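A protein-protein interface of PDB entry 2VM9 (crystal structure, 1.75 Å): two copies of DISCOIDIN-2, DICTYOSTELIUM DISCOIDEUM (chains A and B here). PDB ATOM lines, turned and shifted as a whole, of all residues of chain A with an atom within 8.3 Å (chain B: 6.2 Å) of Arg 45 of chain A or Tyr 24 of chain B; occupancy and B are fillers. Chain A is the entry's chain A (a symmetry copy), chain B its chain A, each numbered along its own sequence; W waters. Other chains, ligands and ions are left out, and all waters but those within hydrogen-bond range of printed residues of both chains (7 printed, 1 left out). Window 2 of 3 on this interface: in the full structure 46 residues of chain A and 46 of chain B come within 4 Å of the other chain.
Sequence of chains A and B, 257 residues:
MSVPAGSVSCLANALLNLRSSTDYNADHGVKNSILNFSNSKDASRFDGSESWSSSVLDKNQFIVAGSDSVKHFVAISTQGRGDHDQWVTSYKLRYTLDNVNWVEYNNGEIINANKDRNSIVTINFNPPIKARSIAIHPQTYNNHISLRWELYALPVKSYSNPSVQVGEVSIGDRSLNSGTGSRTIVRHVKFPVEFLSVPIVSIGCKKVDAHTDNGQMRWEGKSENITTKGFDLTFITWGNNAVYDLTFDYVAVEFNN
OD2 of Asp 47 of chain A lies within hydrogen-bond range of OG of Ser 55 of chain B (2.5 Å). NH1 of Arg 45 of chain A lies within hydrogen-bond range of OG of Ser 55 of chain B (2.9 Å). The backbone NH (N) of Ala 26 of chain B is in hydrogen-bond range of the side-chain carboxylate (OD1) of Asp 27 of chain A (2.7 Å). O of Asp 47 of chain A sits close to O of Asp 23 of chain B (3.5 Å). OD2 of Asp 23 of chain B lies within salt-bridge range of NZ of Lys 31 of chain A, at 2.8 Å.
NE of Arg 45 of chain A is in salt-bridge range of OD2 of Asp 42 of chain A, at 3.6 Å. N of Tyr 24 of chain B lies within hydrogen-bond range of O of Ser 54 of chain B, at 3.3 Å. The backbone carbonyl oxygen of Thr 22 of chain B sits at hydrogen-bond distance from the indole nitrogen of Trp 52 of chain B (2.9 Å). OD1 of Asn 25 of chain B is in hydrogen-bond range of ND1 of His 28 of chain B, at 2.8 Å. The side-chain hydroxyl (OG1) of Thr 22 of chain B is in hydrogen-bond range of the backbone NH (N) of Val 56 of chain B, 3.2 Å away. OG of Ser 40 of chain A is in hydrogen-bond range of N of Asp 42 of chain A (3.0 Å).
Among the printed residues, merely in contact across the chains: Asp 27 of chain A with Asn 25 of chain B (3.4 Å), Lys 31 of chain A with Ala 26 of chain B (3.7 Å), Asn 39 of chain A with Thr 22 of chain B (3.9 Å), Ser 40 of chain A with Ser 55 of chain B (3.4 Å), Ser 40 of chain A with Val 56 of chain B (3.9 Å), Arg 45 of chain A with Tyr 24 of chain B (3.4 Å), Asp 47 of chain A with Tyr 24 of chain B (3.1 Å) and Asp 47 of chain A with Asn 25 of chain B (3.9 Å).
Arg 45 of chain A touches two residues of chain B. Tyr 24 of chain B touches just these residues of chain A: Arg 45 and Asp 47. Of chain A, only Asp 27 and Asp 47 come within 4 Å of Asn 25 of chain B. Printed residues of chain A within 4 Å of Ser 55 of chain B: Ser 40, Arg 45 and Asp 47. Printed residues of chain B within 4 Å of Lys 31 of chain A: Asp 23 (2.8 Å) and Ala 26 (3.7 Å). Of the printed residues of chain A, Val 56 of chain B touches Ser 40 (3.9 Å). Printed residues of chain A within 4 Å of Asp 23 of chain B: Lys 31 and Asp 47. Asp 42 of chain A touches none of the printed residues of chain B. The nearest residue of chain A that does not touch Tyr 24 of chain B is Phe 46 of chain A (4.3 Å).
Of the 13 printed residues of chain B, 7 touch a printed residue of chain A. Hydrophobic or aromatic side chains of chain B within 4 Å of the printed part of chain A: Tyr 24, Ala 26 and Val 56. Printed residues of chain A that touch a printed residue of chain B: Asp 27, Lys 31, Asn 39, Ser 40, Arg 45 and Asp 47. Along chain A the printed residues that touch a printed residue of chain B span positions 27 to 47. Among the printed residues, 13 pairs touch across the chains. Among the printed residues, Asp or Glu carboxylates within 4 Å of a Lys or Arg side-chain nitrogen of the other chain: Lys 31 of chain A with Asp 23 of chain B.
No position is printed for both chains. Of the 13 pairs that touch across the chains among the printed residues, none has its exchanged pair printed and touching as well.
Water W4 bridges the backbone carbonyl oxygen (O) of Ser 55 of chain B (2.6 Å) and the guanidinium group (NH2) of Arg 45 of chain A (3.2 Å). Water W7 bridges O of Tyr 24 of chain B and NH1 of Arg 45 of chain A. Water W2 bridges OH of Tyr 24 of chain B and NE of Arg 45 of chain A. Water W1 lies within hydrogen-bond range of OD2 of Asp 27 of chain A, N of Ala 26 of chain B and OD1 of Asn 25 of chain B. Water W3 lies within hydrogen-bond range of the side-chain amino group of Lys 31 of chain A and the side-chain carboxylate of Asp 23 of chain B. Water W6 bridges O of Phe 46 of chain A (3.2 Å) and ND2 of Asn 25 of chain B (3.4 Å).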
ATOM      1  N   ASP A  27      12.433  20.622   7.627  1.00  0.00           N
ATOM      2  CA  ASP A  27      11.839  20.908   8.928  1.00  0.00           C
ATOM      3  C   ASP A  27      10.320  20.591   9.027  1.00  0.00           C
ATOM      4  O   ASP A  27       9.736  20.761  10.083  1.00  0.00           O
ATOM      5  CB  ASP A  27      12.133  22.345   9.372  1.00  0.00           C
ATOM      6  CG  ASP A  27      13.500  22.480   9.998  1.00  0.00           C
ATOM      7  OD1 ASP A  27      13.900  21.570  10.749  1.00  0.00           O
ATOM      8  OD2 ASP A  27      14.137  23.525   9.745  1.00  0.00           O
ATOM      9  N   LYS A  31      10.073  12.720   9.688  1.00  0.00           N
ATOM     10  CA  LYS A  31      10.715  12.510  10.978  1.00  0.00           C
ATOM     11  C   LYS A  31       9.944  13.268  12.092  1.00  0.00           C
ATOM     12  O   LYS A  31      10.099  12.965  13.288  1.00  0.00           O
ATOM     13  CB  LYS A  31      12.168  12.977  10.926  1.00  0.00           C
ATOM     14  CG  LYS A  31      12.304  14.520  10.832  1.00  0.00           C
ATOM     15  CD  LYS A  31      13.789  14.962  10.921  1.00  0.00           C
ATOM     16  CE  LYS A  31      13.879  16.479  11.035  1.00  0.00           C
ATOM     17  NZ  LYS A  31      13.397  16.966  12.407  1.00  0.00           N
ATOM     18  N   ASN A  39       7.670  19.613  20.121  1.00  0.00           N
ATOM     19  CA  ASN A  39       9.045  20.066  20.306  1.00  0.00           C
ATOM     20  C   ASN A  39       9.056  21.359  21.134  1.00  0.00           C
ATOM     21  O   ASN A  39       8.159  21.537  21.991  1.00  0.00           O
ATOM     22  CB  ASN A  39       9.840  20.085  18.992  1.00  0.00           C
ATOM     23  CG  ASN A  39       9.186  20.963  17.923  1.00  0.00           C
ATOM     24  OD1 ASN A  39       8.347  21.813  18.239  1.00  0.00           O
ATOM     25  ND2 ASN A  39       9.578  20.768  16.665  1.00  0.00           N
ATOM     26  N   SER A  40      10.041  22.228  20.942  1.00  0.00           N
ATOM     27  CA  SER A  40      10.162  23.378  21.833  1.00  0.00           C
ATOM     28  C   SER A  40       8.948  24.294  21.719  1.00  0.00           C
ATOM     29  O   SER A  40       8.419  24.517  20.615  1.00  0.00           O
ATOM     30  CB  SER A  40      11.439  24.165  21.554  1.00  0.00           C
ATOM     31  OG  SER A  40      11.508  25.266  22.446  1.00  0.00           O
ATOM     32  N   LYS A  41       8.515  24.820  22.863  1.00  0.00           N
ATOM     33  CA  LYS A  41       7.476  25.851  22.851  1.00  0.00           C
ATOM     34  C   LYS A  41       8.019  27.268  22.657  1.00  0.00           C
ATOM     35  O   LYS A  41       7.234  28.217  22.530  1.00  0.00           O
ATOM     36  CB  LYS A  41       6.584  25.733  24.093  1.00  0.00           C
ATOM     37  CG  LYS A  41       5.903  24.369  24.219  1.00  0.00           C
ATOM     38  CD  LYS A  41       4.836  24.175  23.161  1.00  0.00           C
ATOM     39  CE  LYS A  41       5.348  23.467  21.910  1.00  0.00           C
ATOM     40  NZ  LYS A  41       4.983  22.031  21.972  1.00  0.00           N
ATOM     41  N   ASP A  42       9.342  27.396  22.565  1.00  0.00           N
ATOM     42  CA  ASP A  42       9.998  28.660  22.334  1.00  0.00           C
ATOM     43  C   ASP A  42       9.496  29.264  21.023  1.00  0.00           C
ATOM     44  O   ASP A  42       9.807  28.774  19.936  1.00  0.00           O
ATOM     45  CB  ASP A  42      11.510  28.458  22.294  1.00  0.00           C
ATOM     46  CG  ASP A  42      12.280  29.757  22.240  1.00  0.00           C
ATOM     47  OD1 ASP A  42      11.682  30.824  21.945  1.00  0.00           O
ATOM     48  OD2 ASP A  42      13.498  29.700  22.502  1.00  0.00           O
ATOM     49  N   ALA A  43       8.714  30.337  21.126  1.00  0.00           N
ATOM     50  CA  ALA A  43       8.138  30.949  19.927  1.00  0.00           C
ATOM     51  C   ALA A  43       9.155  31.755  19.100  1.00  0.00           C
ATOM     52  O   ALA A  43       8.855  32.195  17.969  1.00  0.00           O
ATOM     53  CB  ALA A  43       6.930  31.803  20.310  1.00  0.00           C
ATOM     54  N   SER A  44      10.363  31.907  19.625  1.00  0.00           N
ATOM     55  CA  SER A  44      11.401  32.720  18.984  1.00  0.00           C
ATOM     56  C   SER A  44      12.268  31.993  17.955  1.00  0.00           C
ATOM     57  O   SER A  44      13.141  32.595  17.317  1.00  0.00           O
ATOM     58  CB  SER A  44      12.303  33.373  20.031  1.00  0.00           C
ATOM     59  OG  SER A  44      13.313  32.497  20.510  1.00  0.00           O
ATOM     60  N   ARG A  45      12.055  30.690  17.810  1.00  0.00           N
ATOM     61  CA  ARG A  45      12.826  29.913  16.858  1.00  0.00           C
ATOM     62  C   ARG A  45      11.960  28.766  16.359  1.00  0.00           C
ATOM     63  O   ARG A  45      11.066  28.307  17.067  1.00  0.00           O
ATOM     64  CB  ARG A  45      14.118  29.369  17.495  1.00  0.00           C
ATOM     65  CG  ARG A  45      13.900  28.376  18.658  1.00  0.00           C
ATOM     66  CD  ARG A  45      15.261  27.887  19.239  1.00  0.00           C
ATOM     67  NE  ARG A  45      15.041  27.161  20.488  1.00  0.00           N
ATOM     68  CZ  ARG A  45      14.883  25.836  20.560  1.00  0.00           C
ATOM     69  NH1 ARG A  45      14.938  25.104  19.457  1.00  0.00           N
ATOM     70  NH2 ARG A  45      14.667  25.252  21.737  1.00  0.00           N
ATOM     71  N   PHE A  46      12.233  28.321  15.142  1.00  0.00           N
ATOM     72  CA  PHE A  46      11.468  27.245  14.527  1.00  0.00           C
ATOM     73  C   PHE A  46      12.333  25.988  14.503  1.00  0.00           C
ATOM     74  O   PHE A  46      13.357  25.943  13.824  1.00  0.00           O
ATOM     75  CB  PHE A  46      11.069  27.643  13.108  1.00  0.00           C
ATOM     76  CG  PHE A  46      10.161  26.659  12.447  1.00  0.00           C
ATOM     77  CD1 PHE A  46       8.901  26.423  12.971  1.00  0.00           C
ATOM     78  CD2 PHE A  46      10.574  25.951  11.315  1.00  0.00           C
ATOM     79  CE1 PHE A  46       8.046  25.497  12.393  1.00  0.00           C
ATOM     80  CE2 PHE A  46       9.714  25.024  10.728  1.00  0.00           C
ATOM     81  CZ  PHE A  46       8.460  24.804  11.257  1.00  0.00           C
ATOM     82  N   ASP A  47      11.918  24.982  15.263  1.00  0.00           N
ATOM     83  CA  ASP A  47      12.656  23.728  15.333  1.00  0.00           C
ATOM     84  C   ASP A  47      11.973  22.609  14.521  1.00  0.00           C
ATOM     85  O   ASP A  47      12.363  21.433  14.608  1.00  0.00           O
ATOM     86  CB  ASP A  47      12.896  23.295  16.780  1.00  0.00           C
ATOM     87  CG  ASP A  47      11.609  23.205  17.628  1.00  0.00           C
ATOM     88  OD1 ASP A  47      10.554  23.718  17.202  1.00  0.00           O
ATOM     89  OD2 ASP A  47      11.686  22.641  18.746  1.00  0.00           O
ATOM     90  N   GLY A  48      10.978  22.991  13.735  1.00  0.00           N
ATOM     91  CA  GLY A  48      10.248  22.056  12.892  1.00  0.00           C
ATOM     92  C   GLY A  48       8.769  22.039  13.229  1.00  0.00           C
ATOM     93  O   GLY A  48       8.369  22.357  14.358  1.00  0.00           O
ATOM     94  N   ASP A  83       1.296  22.613  16.053  1.00  0.00           N
ATOM     95  CA  ASP A  83       1.685  24.013  16.227  1.00  0.00           C
ATOM     96  C   ASP A  83       0.994  25.009  15.273  1.00  0.00           C
ATOM     97  O   ASP A  83       1.250  26.223  15.345  1.00  0.00           O
ATOM     98  CB  ASP A  83       3.208  24.156  16.107  1.00  0.00           C
ATOM     99  CG  ASP A  83       3.743  23.705  14.758  1.00  0.00           C
ATOM    100  OD1 ASP A  83       3.431  22.574  14.318  1.00  0.00           O
ATOM    101  OD2 ASP A  83       4.473  24.489  14.144  1.00  0.00           O
ATOM    102  N   THR B  22      13.416  15.151  20.000  1.00  0.00           N
ATOM    103  CA  THR B  22      13.307  16.452  19.323  1.00  0.00           C
ATOM    104  C   THR B  22      14.649  16.702  18.626  1.00  0.00           C
ATOM    105  O   THR B  22      15.673  16.070  18.985  1.00  0.00           O
ATOM    106  CB  THR B  22      13.014  17.632  20.309  1.00  0.00           C
ATOM    107  OG1 THR B  22      14.139  17.826  21.194  1.00  0.00           O
ATOM    108  CG2 THR B  22      11.723  17.369  21.137  1.00  0.00           C
ATOM    109  N   ASP B  23      14.624  17.623  17.658  1.00  0.00           N
ATOM    110  CA  ASP B  23      15.815  18.033  16.883  1.00  0.00           C
ATOM    111  C   ASP B  23      15.862  19.551  16.947  1.00  0.00           C
ATOM    112  O   ASP B  23      14.845  20.212  16.725  1.00  0.00           O
ATOM    113  CB  ASP B  23      15.656  17.684  15.402  1.00  0.00           C
ATOM    114  CG  ASP B  23      15.779  16.203  15.116  1.00  0.00           C
ATOM    115  OD1 ASP B  23      16.350  15.450  15.956  1.00  0.00           O
ATOM    116  OD2 ASP B  23      15.322  15.807  14.009  1.00  0.00           O
ATOM    117  N   TYR B  24      17.041  20.114  17.205  1.00  0.00           N
ATOM    118  CA  TYR B  24      17.143  21.572  17.172  1.00  0.00           C
ATOM    119  C   TYR B  24      16.560  22.121  15.864  1.00  0.00           C
ATOM    120  O   TYR B  24      15.851  23.139  15.844  1.00  0.00           O
ATOM    121  CB  TYR B  24      18.595  22.009  17.322  1.00  0.00           C
ATOM    122  CG  TYR B  24      18.627  23.453  17.710  1.00  0.00           C
ATOM    123  CD1 TYR B  24      18.382  23.828  19.038  1.00  0.00           C
ATOM    124  CD2 TYR B  24      18.877  24.439  16.763  1.00  0.00           C
ATOM    125  CE1 TYR B  24      18.371  25.177  19.412  1.00  0.00           C
ATOM    126  CE2 TYR B  24      18.870  25.801  17.126  1.00  0.00           C
ATOM    127  CZ  TYR B  24      18.606  26.147  18.444  1.00  0.00           C
ATOM    128  OH  TYR B  24      18.625  27.482  18.827  1.00  0.00           O
ATOM    129  N   ASN B  25      16.877  21.425  14.771  1.00  0.00           N
ATOM    130  CA  ASN B  25      16.126  21.508  13.516  1.00  0.00           C
ATOM    131  C   ASN B  25      16.652  20.360  12.655  1.00  0.00           C
ATOM    132  O   ASN B  25      17.410  19.522  13.135  1.00  0.00           O
ATOM    133  CB  ASN B  25      16.312  22.863  12.816  1.00  0.00           C
ATOM    134  CG  ASN B  25      17.762  23.215  12.592  1.00  0.00           C
ATOM    135  OD1 ASN B  25      18.591  22.355  12.287  1.00  0.00           O
ATOM    136  ND2 ASN B  25      18.084  24.500  12.741  1.00  0.00           N
ATOM    137  N   ALA B  26      16.212  20.286  11.404  1.00  0.00           N
ATOM    138  CA  ALA B  26      16.547  19.109  10.576  1.00  0.00           C
ATOM    139  C   ALA B  26      18.043  19.073  10.298  1.00  0.00           C
ATOM    140  O   ALA B  26      18.609  18.000  10.124  1.00  0.00           O
ATOM    141  CB  ALA B  26      15.734  19.109   9.252  1.00  0.00           C
ATOM    142  N   HIS B  28      20.181  19.446  12.452  1.00  0.00           N
ATOM    143  CA  HIS B  28      20.783  18.835  13.653  1.00  0.00           C
ATOM    144  C   HIS B  28      20.127  17.468  13.940  1.00  0.00           C
ATOM    145  O   HIS B  28      20.139  16.994  15.086  1.00  0.00           O
ATOM    146  CB  HIS B  28      20.576  19.741  14.892  1.00  0.00           C
ATOM    147  CG  HIS B  28      21.258  21.076  14.799  1.00  0.00           C
ATOM    148  ND1 HIS B  28      20.786  22.100  14.005  1.00  0.00           N
ATOM    149  CD2 HIS B  28      22.332  21.579  15.465  1.00  0.00           C
ATOM    150  CE1 HIS B  28      21.570  23.161  14.144  1.00  0.00           C
ATOM    151  NE2 HIS B  28      22.519  22.870  15.021  1.00  0.00           N
ATOM    152  N   GLY B  29      19.583  16.824  12.901  1.00  0.00           N
ATOM    153  CA  GLY B  29      18.812  15.575  13.093  1.00  0.00           C
ATOM    154  C   GLY B  29      19.654  14.328  13.313  1.00  0.00           C
ATOM    155  O   GLY B  29      20.890  14.364  13.186  1.00  0.00           O
ATOM    156  N   TRP B  52      23.721  14.613  16.262  1.00  0.00           N
ATOM    157  CA  TRP B  52      22.310  14.932  16.528  1.00  0.00           C
ATOM    158  C   TRP B  52      22.339  15.973  17.654  1.00  0.00           C
ATOM    159  O   TRP B  52      23.115  15.826  18.618  1.00  0.00           O
ATOM    160  CB  TRP B  52      21.567  13.700  17.037  1.00  0.00           C
ATOM    161  CG  TRP B  52      20.271  14.056  17.739  1.00  0.00           C
ATOM    162  CD1 TRP B  52      19.169  14.652  17.174  1.00  0.00           C
ATOM    163  CD2 TRP B  52      19.944  13.820  19.114  1.00  0.00           C
ATOM    164  NE1 TRP B  52      18.180  14.800  18.116  1.00  0.00           N
ATOM    165  CE2 TRP B  52      18.621  14.313  19.319  1.00  0.00           C
ATOM    166  CE3 TRP B  52      20.634  13.253  20.195  1.00  0.00           C
ATOM    167  CZ2 TRP B  52      17.966  14.234  20.560  1.00  0.00           C
ATOM    168  CZ3 TRP B  52      19.981  13.188  21.452  1.00  0.00           C
ATOM    169  CH2 TRP B  52      18.667  13.666  21.614  1.00  0.00           C
ATOM    170  N   SER B  53      21.493  16.999  17.565  1.00  0.00           N
ATOM    171  CA  SER B  53      21.326  17.922  18.713  1.00  0.00           C
ATOM    172  C   SER B  53      19.830  18.080  18.993  1.00  0.00           C
ATOM    173  O   SER B  53      19.056  18.388  18.059  1.00  0.00           O
ATOM    174  CB  SER B  53      21.939  19.296  18.410  1.00  0.00           C
ATOM    175  OG  SER B  53      23.332  19.201  18.119  1.00  0.00           O
ATOM    176  N   SER B  54      19.425  17.911  20.258  1.00  0.00           N
ATOM    177  CA  SER B  54      18.006  18.005  20.606  1.00  0.00           C
ATOM    178  C   SER B  54      17.505  19.448  20.439  1.00  0.00           C
ATOM    179  O   SER B  54      18.289  20.384  20.281  1.00  0.00           O
ATOM    180  CB  SER B  54      17.760  17.529  22.049  1.00  0.00           C
ATOM    181  OG  SER B  54      18.234  18.506  22.950  1.00  0.00           O
ATOM    182  N   SER B  55      16.188  19.625  20.494  1.00  0.00           N
ATOM    183  CA  SER B  55      15.647  20.976  20.589  1.00  0.00           C
ATOM    184  C   SER B  55      15.450  21.412  22.050  1.00  0.00           C
ATOM    185  O   SER B  55      15.893  22.491  22.468  1.00  0.00           O
ATOM    186  CB  SER B  55      14.337  21.122  19.816  1.00  0.00           C
ATOM    187  OG  SER B  55      13.909  22.485  19.915  1.00  0.00           O
ATOM    188  N   VAL B  56      14.797  20.550  22.814  1.00  0.00           N
ATOM    189  CA  VAL B  56      14.532  20.756  24.244  1.00  0.00           C
ATOM    190  C   VAL B  56      15.707  20.228  25.051  1.00  0.00           C
ATOM    191  O   VAL B  56      16.245  19.169  24.751  1.00  0.00           O
ATOM    192  CB  VAL B  56      13.244  19.997  24.621  1.00  0.00           C
ATOM    193  CG1 VAL B  56      13.017  20.030  26.152  1.00  0.00           C
ATOM    194  CG2 VAL B  56      12.069  20.616  23.856  1.00  0.00           C
ATOM    195  N   HIS B 144      24.870  21.495  25.438  1.00  0.00           N
ATOM    196  CA  HIS B 144      23.671  21.051  24.707  1.00  0.00           C
ATOM    197  C   HIS B 144      23.666  19.544  24.619  1.00  0.00           C
ATOM    198  O   HIS B 144      24.722  18.931  24.656  1.00  0.00           O
ATOM    199  CB  HIS B 144      23.683  21.626  23.280  1.00  0.00           C
ATOM    200  CG  HIS B 144      22.317  21.733  22.676  1.00  0.00           C
ATOM    201  ND1 HIS B 144      21.548  22.872  22.784  1.00  0.00           N
ATOM    202  CD2 HIS B 144      21.573  20.835  21.994  1.00  0.00           C
ATOM    203  CE1 HIS B 144      20.395  22.683  22.166  1.00  0.00           C
ATOM    204  NE2 HIS B 144      20.381  21.447  21.692  1.00  0.00           N
HETATM  205  O   HOH W   1      16.915  22.843   9.543  1.00  0.00           O
HETATM  206  O   HOH W   2      18.067  28.123  21.556  1.00  0.00           O
HETATM  207  O   HOH W   3      12.286  16.908  15.184  1.00  0.00           O
HETATM  208  O   HOH W   4      17.051  24.406  23.771  1.00  0.00           O
HETATM  209  O   HOH W   5      12.125  19.083  16.729  1.00  0.00           O
HETATM  210  O   HOH W   6      16.385  26.664  14.667  1.00  0.00           O
HETATM  211  O   HOH W   7      15.393  25.722  16.764  1.00  0.00           O
